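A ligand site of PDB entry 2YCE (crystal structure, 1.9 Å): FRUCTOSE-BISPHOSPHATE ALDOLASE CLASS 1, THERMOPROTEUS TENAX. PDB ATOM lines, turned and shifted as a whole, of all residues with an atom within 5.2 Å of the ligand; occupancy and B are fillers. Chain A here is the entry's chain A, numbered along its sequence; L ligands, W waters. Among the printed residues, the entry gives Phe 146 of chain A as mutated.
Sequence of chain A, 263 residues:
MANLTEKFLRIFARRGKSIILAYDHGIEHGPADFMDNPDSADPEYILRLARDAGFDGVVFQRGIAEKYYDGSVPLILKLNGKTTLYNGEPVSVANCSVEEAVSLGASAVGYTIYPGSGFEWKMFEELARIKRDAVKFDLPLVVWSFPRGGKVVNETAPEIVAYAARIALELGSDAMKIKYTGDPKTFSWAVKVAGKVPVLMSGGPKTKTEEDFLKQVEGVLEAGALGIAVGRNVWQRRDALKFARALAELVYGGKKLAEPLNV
Ala 22 touches the ligand (CB to C1, 3.6 Å). Phe 146 touches the ligand. Ala 229 touches the ligand. Val 230 touches the ligand (CA to O3, 3.4 Å). Hydrophobic or aromatic side chains that line the ligand: Ala 22, His 25, His 29, Trp 144 and Phe 146.
Water W3 lies within hydrogen-bond range of an oxygen (O3) of the ligand (2.5 Å), the backbone carbonyl oxygen (O) of Gly 204 (2.7 Å), the backbone NH (N) of Asn 233 (2.8 Å) and the backbone NH (N) of Arg 232 (3.4 Å). Water W2 lies within hydrogen-bond range of O12 of the ligand (2.6 Å) and NH2 of Arg 148 (3.5 Å). Water W7 lies within hydrogen-bond range of O10 of the ligand (2.6 Å) and NH2 of Arg 232 (3.1 Å). Water W1 lies within hydrogen-bond range of O10 of the ligand and NE2 of His 29. Water W4 lies within hydrogen-bond range of OG1 of Thr 112 and O7 of the ligand. Water W6 lies within hydrogen-bond range of the side-chain hydroxyl of Tyr 114 (2.5 Å), the side-chain carboxylate of Glu 28 (2.7 Å) and an oxygen (O11) of the ligand (2.9 Å).
NZ of Lys 177 is covalently linked to C6 of the ligand, 1.6 Å away. An oxygen (O10) of the ligand sits at hydrogen-bond distance from a ring nitrogen (NE2) of His 29, at 2.6 Å. The side-chain carboxylate (OD1) of Asp 24 sits at hydrogen-bond distance from an oxygen (O6) of the ligand. NE2 of His 25 sits at hydrogen-bond distance from O1 of the ligand (2.7 Å). OG of Ser 202 lies within hydrogen-bond range of O5 of the ligand, at 2.7 Å. The guanidinium group (NH1) of Arg 148 lies within salt-bridge range of an oxygen (O11) of the ligand. O12 of the ligand is in salt-bridge range of NZ of Lys 179, 2.8 Å away. An oxygen (O2) of the ligand lies within hydrogen-bond range of the backbone NH of Gly 204 (2.8 Å). An oxygen (O3) of the ligand is in hydrogen-bond range of the backbone NH (N) of Gly 231 (2.8 Å). N of Arg 232 lies within hydrogen-bond range of O1 of the ligand (2.8 Å). An oxygen (O1) of the ligand is in salt-bridge range of the guanidinium group (NE) of Arg 232 (2.8 Å). The backbone NH (N) of Gly 203 sits close to an oxygen (O3) of the ligand (3.3 Å). The indole nitrogen of Trp 144 sits at hydrogen-bond distance from an oxygen (O7) of the ligand (3.2 Å).
The side-chain carboxylate (OD1) of Asp 24 sits at hydrogen-bond distance from a ring nitrogen (ND1) of His 25 (3.5 Å). NE of Arg 148 lies within salt-bridge range of OE2 of Glu 155 (2.9 Å). O of Gly 204 sits at hydrogen-bond distance from ND2 of Asn 233. The backbone carbonyl oxygen (O) of Gly 231 sits close to the indole nitrogen (NE1) of Trp 235, at 3.4 Å. The backbone carbonyl oxygen (O) of Ala 229 sits at hydrogen-bond distance from the backbone NH (N) of Gly 203, 3.1 Å away. O of Gly 203 lies within hydrogen-bond range of ND2 of Asn 233. The backbone NH (N) of Ala 22 is in hydrogen-bond range of the backbone carbonyl oxygen (O) of Val 230, at 2.8 Å. The indole nitrogen (NE1) of Trp 235 lies within hydrogen-bond range of the backbone carbonyl oxygen (O) of Ala 22, 3.0 Å away.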
ATOM      1  N   ALA A  22     -19.053 -21.419  30.877  1.00  0.00           N
ATOM      2  CA  ALA A  22     -17.850 -20.638  31.257  1.00  0.00           C
ATOM      3  C   ALA A  22     -17.919 -19.256  30.604  1.00  0.00           C
ATOM      4  O   ALA A  22     -18.300 -19.154  29.431  1.00  0.00           O
ATOM      5  CB  ALA A  22     -16.621 -21.366  30.843  1.00  0.00           C
ATOM      6  N   ASP A  24     -15.505 -16.294  31.432  1.00  0.00           N
ATOM      7  CA  ASP A  24     -14.370 -15.454  31.789  1.00  0.00           C
ATOM      8  C   ASP A  24     -13.683 -14.898  30.524  1.00  0.00           C
ATOM      9  O   ASP A  24     -12.619 -14.233  30.613  1.00  0.00           O
ATOM     10  CB  ASP A  24     -13.338 -16.204  32.693  1.00  0.00           C
ATOM     11  CG  ASP A  24     -12.748 -17.454  32.020  1.00  0.00           C
ATOM     12  OD1 ASP A  24     -13.438 -18.032  31.140  1.00  0.00           O
ATOM     13  OD2 ASP A  24     -11.592 -17.878  32.361  1.00  0.00           O
ATOM     14  N   HIS A  25     -14.290 -15.123  29.352  1.00  0.00           N
ATOM     15  CA  HIS A  25     -13.629 -14.841  28.066  1.00  0.00           C
ATOM     16  C   HIS A  25     -13.402 -13.352  27.814  1.00  0.00           C
ATOM     17  O   HIS A  25     -12.455 -12.955  27.086  1.00  0.00           O
ATOM     18  CB  HIS A  25     -14.423 -15.456  26.907  1.00  0.00           C
ATOM     19  CG  HIS A  25     -14.594 -16.939  27.048  1.00  0.00           C
ATOM     20  ND1 HIS A  25     -15.153 -17.504  28.189  1.00  0.00           N
ATOM     21  CD2 HIS A  25     -14.266 -17.963  26.227  1.00  0.00           C
ATOM     22  CE1 HIS A  25     -15.156 -18.824  28.055  1.00  0.00           C
ATOM     23  NE2 HIS A  25     -14.623 -19.123  26.875  1.00  0.00           N
ATOM     24  N   GLU A  28      -9.974 -12.894  29.258  1.00  0.00           N
ATOM     25  CA  GLU A  28      -8.962 -13.829  28.712  1.00  0.00           C
ATOM     26  C   GLU A  28      -8.698 -13.637  27.221  1.00  0.00           C
ATOM     27  O   GLU A  28      -7.524 -13.674  26.802  1.00  0.00           O
ATOM     28  CB  GLU A  28      -9.335 -15.297  29.004  1.00  0.00           C
ATOM     29  CG  GLU A  28      -9.332 -15.690  30.450  1.00  0.00           C
ATOM     30  CD  GLU A  28      -7.920 -15.731  31.060  1.00  0.00           C
ATOM     31  OE1 GLU A  28      -6.959 -16.086  30.365  1.00  0.00           O
ATOM     32  OE2 GLU A  28      -7.779 -15.424  32.267  1.00  0.00           O
ATOM     33  N   HIS A  29      -9.781 -13.393  26.440  1.00  0.00           N
ATOM     34  CA  HIS A  29      -9.668 -13.245  24.977  1.00  0.00           C
ATOM     35  C   HIS A  29     -10.152 -11.930  24.453  1.00  0.00           C
ATOM     36  O   HIS A  29      -9.787 -11.528  23.343  1.00  0.00           O
ATOM     37  CB  HIS A  29     -10.413 -14.370  24.224  1.00  0.00           C
ATOM     38  CG  HIS A  29      -9.988 -15.745  24.639  1.00  0.00           C
ATOM     39  ND1 HIS A  29     -10.881 -16.787  24.766  1.00  0.00           N
ATOM     40  CD2 HIS A  29      -8.782 -16.241  24.998  1.00  0.00           C
ATOM     41  CE1 HIS A  29     -10.228 -17.869  25.164  1.00  0.00           C
ATOM     42  NE2 HIS A  29      -8.958 -17.570  25.297  1.00  0.00           N
ATOM     43  N   LYS A  78     -14.343 -16.743  39.208  1.00  0.00           N
ATOM     44  CA  LYS A  78     -12.998 -16.953  38.693  1.00  0.00           C
ATOM     45  C   LYS A  78     -12.129 -15.792  39.184  1.00  0.00           C
ATOM     46  O   LYS A  78     -12.302 -14.645  38.755  1.00  0.00           O
ATOM     47  CB  LYS A  78     -13.016 -17.052  37.156  1.00  0.00           C
ATOM     48  CG  LYS A  78     -11.653 -17.221  36.470  1.00  0.00           C
ATOM     49  CD  LYS A  78     -10.961 -18.545  36.919  1.00  0.00           C
ATOM     50  CE  LYS A  78      -9.983 -19.054  35.845  1.00  0.00           C
ATOM     51  NZ  LYS A  78      -8.923 -18.011  35.565  1.00  0.00           N
ATOM     52  N   THR A 112      -6.708 -20.225  37.717  1.00  0.00           N
ATOM     53  CA  THR A 112      -5.808 -20.800  36.722  1.00  0.00           C
ATOM     54  C   THR A 112      -4.320 -20.840  37.134  1.00  0.00           C
ATOM     55  O   THR A 112      -3.747 -19.865  37.655  1.00  0.00           O
ATOM     56  CB  THR A 112      -5.895 -20.071  35.367  1.00  0.00           C
ATOM     57  OG1 THR A 112      -7.261 -20.029  34.944  1.00  0.00           O
ATOM     58  CG2 THR A 112      -5.026 -20.781  34.284  1.00  0.00           C
ATOM     59  N   TYR A 114      -0.452 -22.097  35.422  1.00  0.00           N
ATOM     60  CA  TYR A 114       0.272 -22.516  34.189  1.00  0.00           C
ATOM     61  C   TYR A 114       1.548 -23.260  34.546  1.00  0.00           C
ATOM     62  O   TYR A 114       2.599 -22.691  34.473  1.00  0.00           O
ATOM     63  CB  TYR A 114       0.592 -21.317  33.242  1.00  0.00           C
ATOM     64  CG  TYR A 114      -0.605 -20.441  32.926  1.00  0.00           C
ATOM     65  CD1 TYR A 114      -1.624 -20.912  32.072  1.00  0.00           C
ATOM     66  CD2 TYR A 114      -0.769 -19.181  33.535  1.00  0.00           C
ATOM     67  CE1 TYR A 114      -2.725 -20.096  31.756  1.00  0.00           C
ATOM     68  CE2 TYR A 114      -1.876 -18.362  33.238  1.00  0.00           C
ATOM     69  CZ  TYR A 114      -2.845 -18.832  32.359  1.00  0.00           C
ATOM     70  OH  TYR A 114      -3.977 -18.087  32.117  1.00  0.00           O
ATOM     71  N   TRP A 144      -8.227 -24.477  37.224  1.00  0.00           N
ATOM     72  CA  TRP A 144      -7.980 -24.625  35.789  1.00  0.00           C
ATOM     73  C   TRP A 144      -6.477 -24.946  35.702  1.00  0.00           C
ATOM     74  O   TRP A 144      -5.640 -24.076  35.936  1.00  0.00           O
ATOM     75  CB  TRP A 144      -8.201 -23.280  35.098  1.00  0.00           C
ATOM     76  CG  TRP A 144      -9.617 -22.767  34.747  1.00  0.00           C
ATOM     77  CD1 TRP A 144      -9.962 -22.218  33.530  1.00  0.00           C
ATOM     78  CD2 TRP A 144     -10.791 -22.625  35.591  1.00  0.00           C
ATOM     79  NE1 TRP A 144     -11.249 -21.791  33.550  1.00  0.00           N
ATOM     80  CE2 TRP A 144     -11.793 -22.037  34.787  1.00  0.00           C
ATOM     81  CE3 TRP A 144     -11.106 -22.971  36.904  1.00  0.00           C
ATOM     82  CZ2 TRP A 144     -13.101 -21.771  35.253  1.00  0.00           C
ATOM     83  CZ3 TRP A 144     -12.422 -22.693  37.387  1.00  0.00           C
ATOM     84  CH2 TRP A 144     -13.383 -22.105  36.554  1.00  0.00           C
ATOM     85  N   PHE A 146      -3.614 -25.585  33.341  1.00  0.00           N
ATOM     86  CA  PHE A 146      -3.249 -25.409  31.910  1.00  0.00           C
ATOM     87  C   PHE A 146      -1.715 -25.244  31.772  1.00  0.00           C
ATOM     88  O   PHE A 146      -1.225 -24.118  31.649  1.00  0.00           O
ATOM     89  CB  PHE A 146      -3.945 -24.141  31.339  1.00  0.00           C
ATOM     90  CG  PHE A 146      -5.463 -24.231  31.225  1.00  0.00           C
ATOM     91  CD1 PHE A 146      -6.148 -25.456  31.282  1.00  0.00           C
ATOM     92  CD2 PHE A 146      -6.210 -23.062  30.962  1.00  0.00           C
ATOM     93  CE1 PHE A 146      -7.568 -25.518  31.145  1.00  0.00           C
ATOM     94  CE2 PHE A 146      -7.621 -23.119  30.795  1.00  0.00           C
ATOM     95  CZ  PHE A 146      -8.295 -24.346  30.888  1.00  0.00           C
ATOM     96  N   ARG A 148       1.735 -24.434  30.390  1.00  0.00           N
ATOM     97  CA  ARG A 148       1.963 -23.439  29.355  1.00  0.00           C
ATOM     98  C   ARG A 148       3.298 -22.745  29.677  1.00  0.00           C
ATOM     99  O   ARG A 148       3.558 -22.423  30.838  1.00  0.00           O
ATOM    100  CB  ARG A 148       0.828 -22.394  29.336  1.00  0.00           C
ATOM    101  CG  ARG A 148       0.776 -21.566  28.043  1.00  0.00           C
ATOM    102  CD  ARG A 148      -0.535 -20.769  27.923  1.00  0.00           C
ATOM    103  NE  ARG A 148      -1.657 -21.658  27.621  1.00  0.00           N
ATOM    104  CZ  ARG A 148      -2.952 -21.369  27.777  1.00  0.00           C
ATOM    105  NH1 ARG A 148      -3.339 -20.188  28.232  1.00  0.00           N
ATOM    106  NH2 ARG A 148      -3.868 -22.279  27.445  1.00  0.00           N
ATOM    107  N   GLU A 155      -0.151 -28.684  24.246  1.00  0.00           N
ATOM    108  CA  GLU A 155      -0.957 -28.648  25.464  1.00  0.00           C
ATOM    109  C   GLU A 155      -1.971 -29.760  25.579  1.00  0.00           C
ATOM    110  O   GLU A 155      -2.527 -30.017  26.663  1.00  0.00           O
ATOM    111  CB  GLU A 155      -1.674 -27.306  25.593  1.00  0.00           C
ATOM    112  CG  GLU A 155      -0.732 -26.146  25.928  1.00  0.00           C
ATOM    113  CD  GLU A 155      -1.495 -24.813  26.042  1.00  0.00           C
ATOM    114  OE1 GLU A 155      -2.679 -24.829  26.456  1.00  0.00           O
ATOM    115  OE2 GLU A 155      -0.898 -23.762  25.733  1.00  0.00           O
ATOM    116  N   LYS A 177     -10.380 -28.353  36.069  1.00  0.00           N
ATOM    117  CA  LYS A 177     -10.687 -28.185  34.667  1.00  0.00           C
ATOM    118  C   LYS A 177      -9.366 -28.331  33.865  1.00  0.00           C
ATOM    119  O   LYS A 177      -8.395 -27.611  34.138  1.00  0.00           O
ATOM    120  CB  LYS A 177     -11.364 -26.829  34.475  1.00  0.00           C
ATOM    121  CG  LYS A 177     -11.644 -26.437  32.994  1.00  0.00           C
ATOM    122  CD  LYS A 177     -12.161 -24.986  32.975  1.00  0.00           C
ATOM    123  CE  LYS A 177     -12.747 -24.679  31.623  1.00  0.00           C
ATOM    124  NZ  LYS A 177     -12.349 -23.406  30.950  1.00  0.00           N
ATOM    125  N   LYS A 179      -7.540 -29.458  29.680  1.00  0.00           N
ATOM    126  CA  LYS A 179      -7.751 -29.648  28.226  1.00  0.00           C
ATOM    127  C   LYS A 179      -8.020 -31.109  27.911  1.00  0.00           C
ATOM    128  O   LYS A 179      -7.499 -32.007  28.599  1.00  0.00           O
ATOM    129  CB  LYS A 179      -6.507 -29.203  27.447  1.00  0.00           C
ATOM    130  CG  LYS A 179      -6.072 -27.768  27.730  1.00  0.00           C
ATOM    131  CD  LYS A 179      -7.133 -26.787  27.393  1.00  0.00           C
ATOM    132  CE  LYS A 179      -6.602 -25.349  27.678  1.00  0.00           C
ATOM    133  NZ  LYS A 179      -7.659 -24.297  27.385  1.00  0.00           N
ATOM    134  N   SER A 202     -12.326 -28.786  29.584  1.00  0.00           N
ATOM    135  CA  SER A 202     -12.330 -27.460  28.963  1.00  0.00           C
ATOM    136  C   SER A 202     -12.847 -27.546  27.501  1.00  0.00           C
ATOM    137  O   SER A 202     -12.297 -28.302  26.697  1.00  0.00           O
ATOM    138  CB  SER A 202     -10.919 -26.848  29.034  1.00  0.00           C
ATOM    139  OG  SER A 202     -10.862 -25.607  28.309  1.00  0.00           O
ATOM    140  N   GLY A 203     -13.884 -26.780  27.152  1.00  0.00           N
ATOM    141  CA  GLY A 203     -14.527 -26.877  25.818  1.00  0.00           C
ATOM    142  C   GLY A 203     -13.631 -26.560  24.611  1.00  0.00           C
ATOM    143  O   GLY A 203     -13.709 -27.242  23.592  1.00  0.00           O
ATOM    144  N   GLY A 204     -12.774 -25.545  24.734  1.00  0.00           N
ATOM    145  CA  GLY A 204     -11.859 -25.150  23.651  1.00  0.00           C
ATOM    146  C   GLY A 204     -12.522 -24.319  22.556  1.00  0.00           C
ATOM    147  O   GLY A 204     -13.715 -24.009  22.649  1.00  0.00           O
ATOM    148  N   PRO A 205     -11.738 -23.922  21.512  1.00  0.00           N
ATOM    149  CA  PRO A 205     -12.315 -23.143  20.413  1.00  0.00           C
ATOM    150  C   PRO A 205     -13.509 -23.869  19.782  1.00  0.00           C
ATOM    151  O   PRO A 205     -13.602 -25.112  19.840  1.00  0.00           O
ATOM    152  CB  PRO A 205     -11.154 -23.033  19.397  1.00  0.00           C
ATOM    153  CG  PRO A 205      -9.920 -23.212  20.201  1.00  0.00           C
ATOM    154  CD  PRO A 205     -10.294 -24.157  21.326  1.00  0.00           C
ATOM    155  N   ALA A 229     -16.876 -27.889  31.202  1.00  0.00           N
ATOM    156  CA  ALA A 229     -16.963 -26.456  31.448  1.00  0.00           C
ATOM    157  C   ALA A 229     -16.787 -25.865  30.058  1.00  0.00           C
ATOM    158  O   ALA A 229     -15.695 -25.915  29.471  1.00  0.00           O
ATOM    159  CB  ALA A 229     -15.847 -25.994  32.402  1.00  0.00           C
ATOM    160  N   VAL A 230     -17.874 -25.339  29.512  1.00  0.00           N
ATOM    161  CA  VAL A 230     -17.931 -24.998  28.098  1.00  0.00           C
ATOM    162  C   VAL A 230     -18.362 -23.551  27.949  1.00  0.00           C
ATOM    163  O   VAL A 230     -19.239 -23.076  28.678  1.00  0.00           O
ATOM    164  CB  VAL A 230     -18.892 -25.960  27.318  1.00  0.00           C
ATOM    165  CG1 VAL A 230     -20.329 -25.953  27.906  1.00  0.00           C
ATOM    166  CG2 VAL A 230     -18.938 -25.635  25.814  1.00  0.00           C
ATOM    167  N   GLY A 231     -17.715 -22.843  27.012  1.00  0.00           N
ATOM    168  CA  GLY A 231     -18.058 -21.462  26.733  1.00  0.00           C
ATOM    169  C   GLY A 231     -18.363 -21.306  25.269  1.00  0.00           C
ATOM    170  O   GLY A 231     -19.531 -21.327  24.862  1.00  0.00           O
ATOM    171  N   ARG A 232     -17.313 -21.199  24.460  1.00  0.00           N
ATOM    172  CA  ARG A 232     -17.441 -20.878  23.045  1.00  0.00           C
ATOM    173  C   ARG A 232     -18.288 -21.904  22.284  1.00  0.00           C
ATOM    174  O   ARG A 232     -19.083 -21.522  21.392  1.00  0.00           O
ATOM    175  CB  ARG A 232     -16.049 -20.725  22.407  1.00  0.00           C
ATOM    176  CG  ARG A 232     -15.299 -19.458  22.839  1.00  0.00           C
ATOM    177  CD  ARG A 232     -13.806 -19.526  22.474  1.00  0.00           C
ATOM    178  NE  ARG A 232     -13.094 -20.417  23.391  1.00  0.00           N
ATOM    179  CZ  ARG A 232     -11.803 -20.702  23.309  1.00  0.00           C
ATOM    180  NH1 ARG A 232     -11.042 -20.168  22.353  1.00  0.00           N
ATOM    181  NH2 ARG A 232     -11.258 -21.524  24.209  1.00  0.00           N
ATOM    182  N   ASN A 233     -18.165 -23.188  22.619  1.00  0.00           N
ATOM    183  CA  ASN A 233     -18.941 -24.199  21.892  1.00  0.00           C
ATOM    184  C   ASN A 233     -20.467 -24.151  22.172  1.00  0.00           C
ATOM    185  O   ASN A 233     -21.240 -24.804  21.488  1.00  0.00           O
ATOM    186  CB  ASN A 233     -18.334 -25.605  22.033  1.00  0.00           C
ATOM    187  CG  ASN A 233     -17.269 -25.874  20.976  1.00  0.00           C
ATOM    188  OD1 ASN A 233     -17.586 -26.076  19.786  1.00  0.00           O
ATOM    189  ND2 ASN A 233     -15.991 -25.845  21.399  1.00  0.00           N
ATOM    190  N   TRP A 235     -22.010 -20.528  23.516  1.00  0.00           N
ATOM    191  CA  TRP A 235     -22.447 -19.155  23.204  1.00  0.00           C
ATOM    192  C   TRP A 235     -21.919 -18.501  21.911  1.00  0.00           C
ATOM    193  O   TRP A 235     -22.464 -17.469  21.504  1.00  0.00           O
ATOM    194  CB  TRP A 235     -22.356 -18.198  24.413  1.00  0.00           C
ATOM    195  CG  TRP A 235     -21.079 -18.154  25.123  1.00  0.00           C
ATOM    196  CD1 TRP A 235     -20.829 -18.667  26.375  1.00  0.00           C
ATOM    197  CD2 TRP A 235     -19.842 -17.583  24.677  1.00  0.00           C
ATOM    198  NE1 TRP A 235     -19.525 -18.432  26.734  1.00  0.00           N
ATOM    199  CE2 TRP A 235     -18.887 -17.762  25.713  1.00  0.00           C
ATOM    200  CE3 TRP A 235     -19.442 -16.920  23.508  1.00  0.00           C
ATOM    201  CZ2 TRP A 235     -17.552 -17.328  25.602  1.00  0.00           C
ATOM    202  CZ3 TRP A 235     -18.091 -16.482  23.412  1.00  0.00           C
ATOM    203  CH2 TRP A 235     -17.179 -16.685  24.458  1.00  0.00           C
HETATM  204  C1  LIG L   1     -13.884 -22.880  29.073  1.00  0.00           C
HETATM  205  C2  LIG L   1     -10.483 -19.487  28.742  1.00  0.00           C
HETATM  206  C3  LIG L   1      -8.973 -19.278  28.685  1.00  0.00           C
HETATM  207  C4  LIG L   1     -10.795 -20.597  29.775  1.00  0.00           C
HETATM  208  C5  LIG L   1     -12.275 -21.045  29.750  1.00  0.00           C
HETATM  209  C6  LIG L   1     -12.462 -22.574  29.614  1.00  0.00           C
HETATM  210  O1  LIG L   1     -14.696 -21.419  25.479  1.00  0.00           O
HETATM  211  P1  LIG L   1     -14.301 -22.629  26.437  1.00  0.00           P
HETATM  212  O2  LIG L   1     -12.809 -23.119  26.125  1.00  0.00           O
HETATM  213  O3  LIG L   1     -15.161 -23.852  26.410  1.00  0.00           O
HETATM  214  O4  LIG L   1     -14.213 -21.994  27.940  1.00  0.00           O
HETATM  215  O5  LIG L   1     -11.534 -23.016  28.651  1.00  0.00           O
HETATM  216  O6  LIG L   1     -12.958 -20.669  30.950  1.00  0.00           O
HETATM  217  O7  LIG L   1     -10.398 -20.084  31.032  1.00  0.00           O
HETATM  218  O8  LIG L   1     -10.882 -19.971  27.480  1.00  0.00           O
HETATM  219  O9  LIG L   1      -8.386 -20.481  28.091  1.00  0.00           O
HETATM  220  P2  LIG L   1      -7.055 -20.428  27.145  1.00  0.00           P
HETATM  221  O10 LIG L   1      -7.552 -19.653  25.872  1.00  0.00           O
HETATM  222  O11 LIG L   1      -5.974 -19.483  27.863  1.00  0.00           O
HETATM  223  O12 LIG L   1      -6.550 -21.809  26.902  1.00  0.00           O
HETATM  224  O   HOH W   1      -5.759 -18.318  24.147  1.00  0.00           O
HETATM  225  O   HOH W   2      -5.744 -22.491  24.537  1.00  0.00           O
HETATM  226  O   HOH W   3     -16.029 -24.348  24.079  1.00  0.00           O
HETATM  227  O   HOH W   4      -7.886 -19.748  32.336  1.00  0.00           O
HETATM  228  O   HOH W   5      -5.522 -17.161  26.483  1.00  0.00           O
HETATM  229  O   HOH W   6      -5.935 -18.528  30.556  1.00  0.00           O
HETATM  230  O   HOH W   7      -8.129 -21.525  24.133  1.00  0.00           O
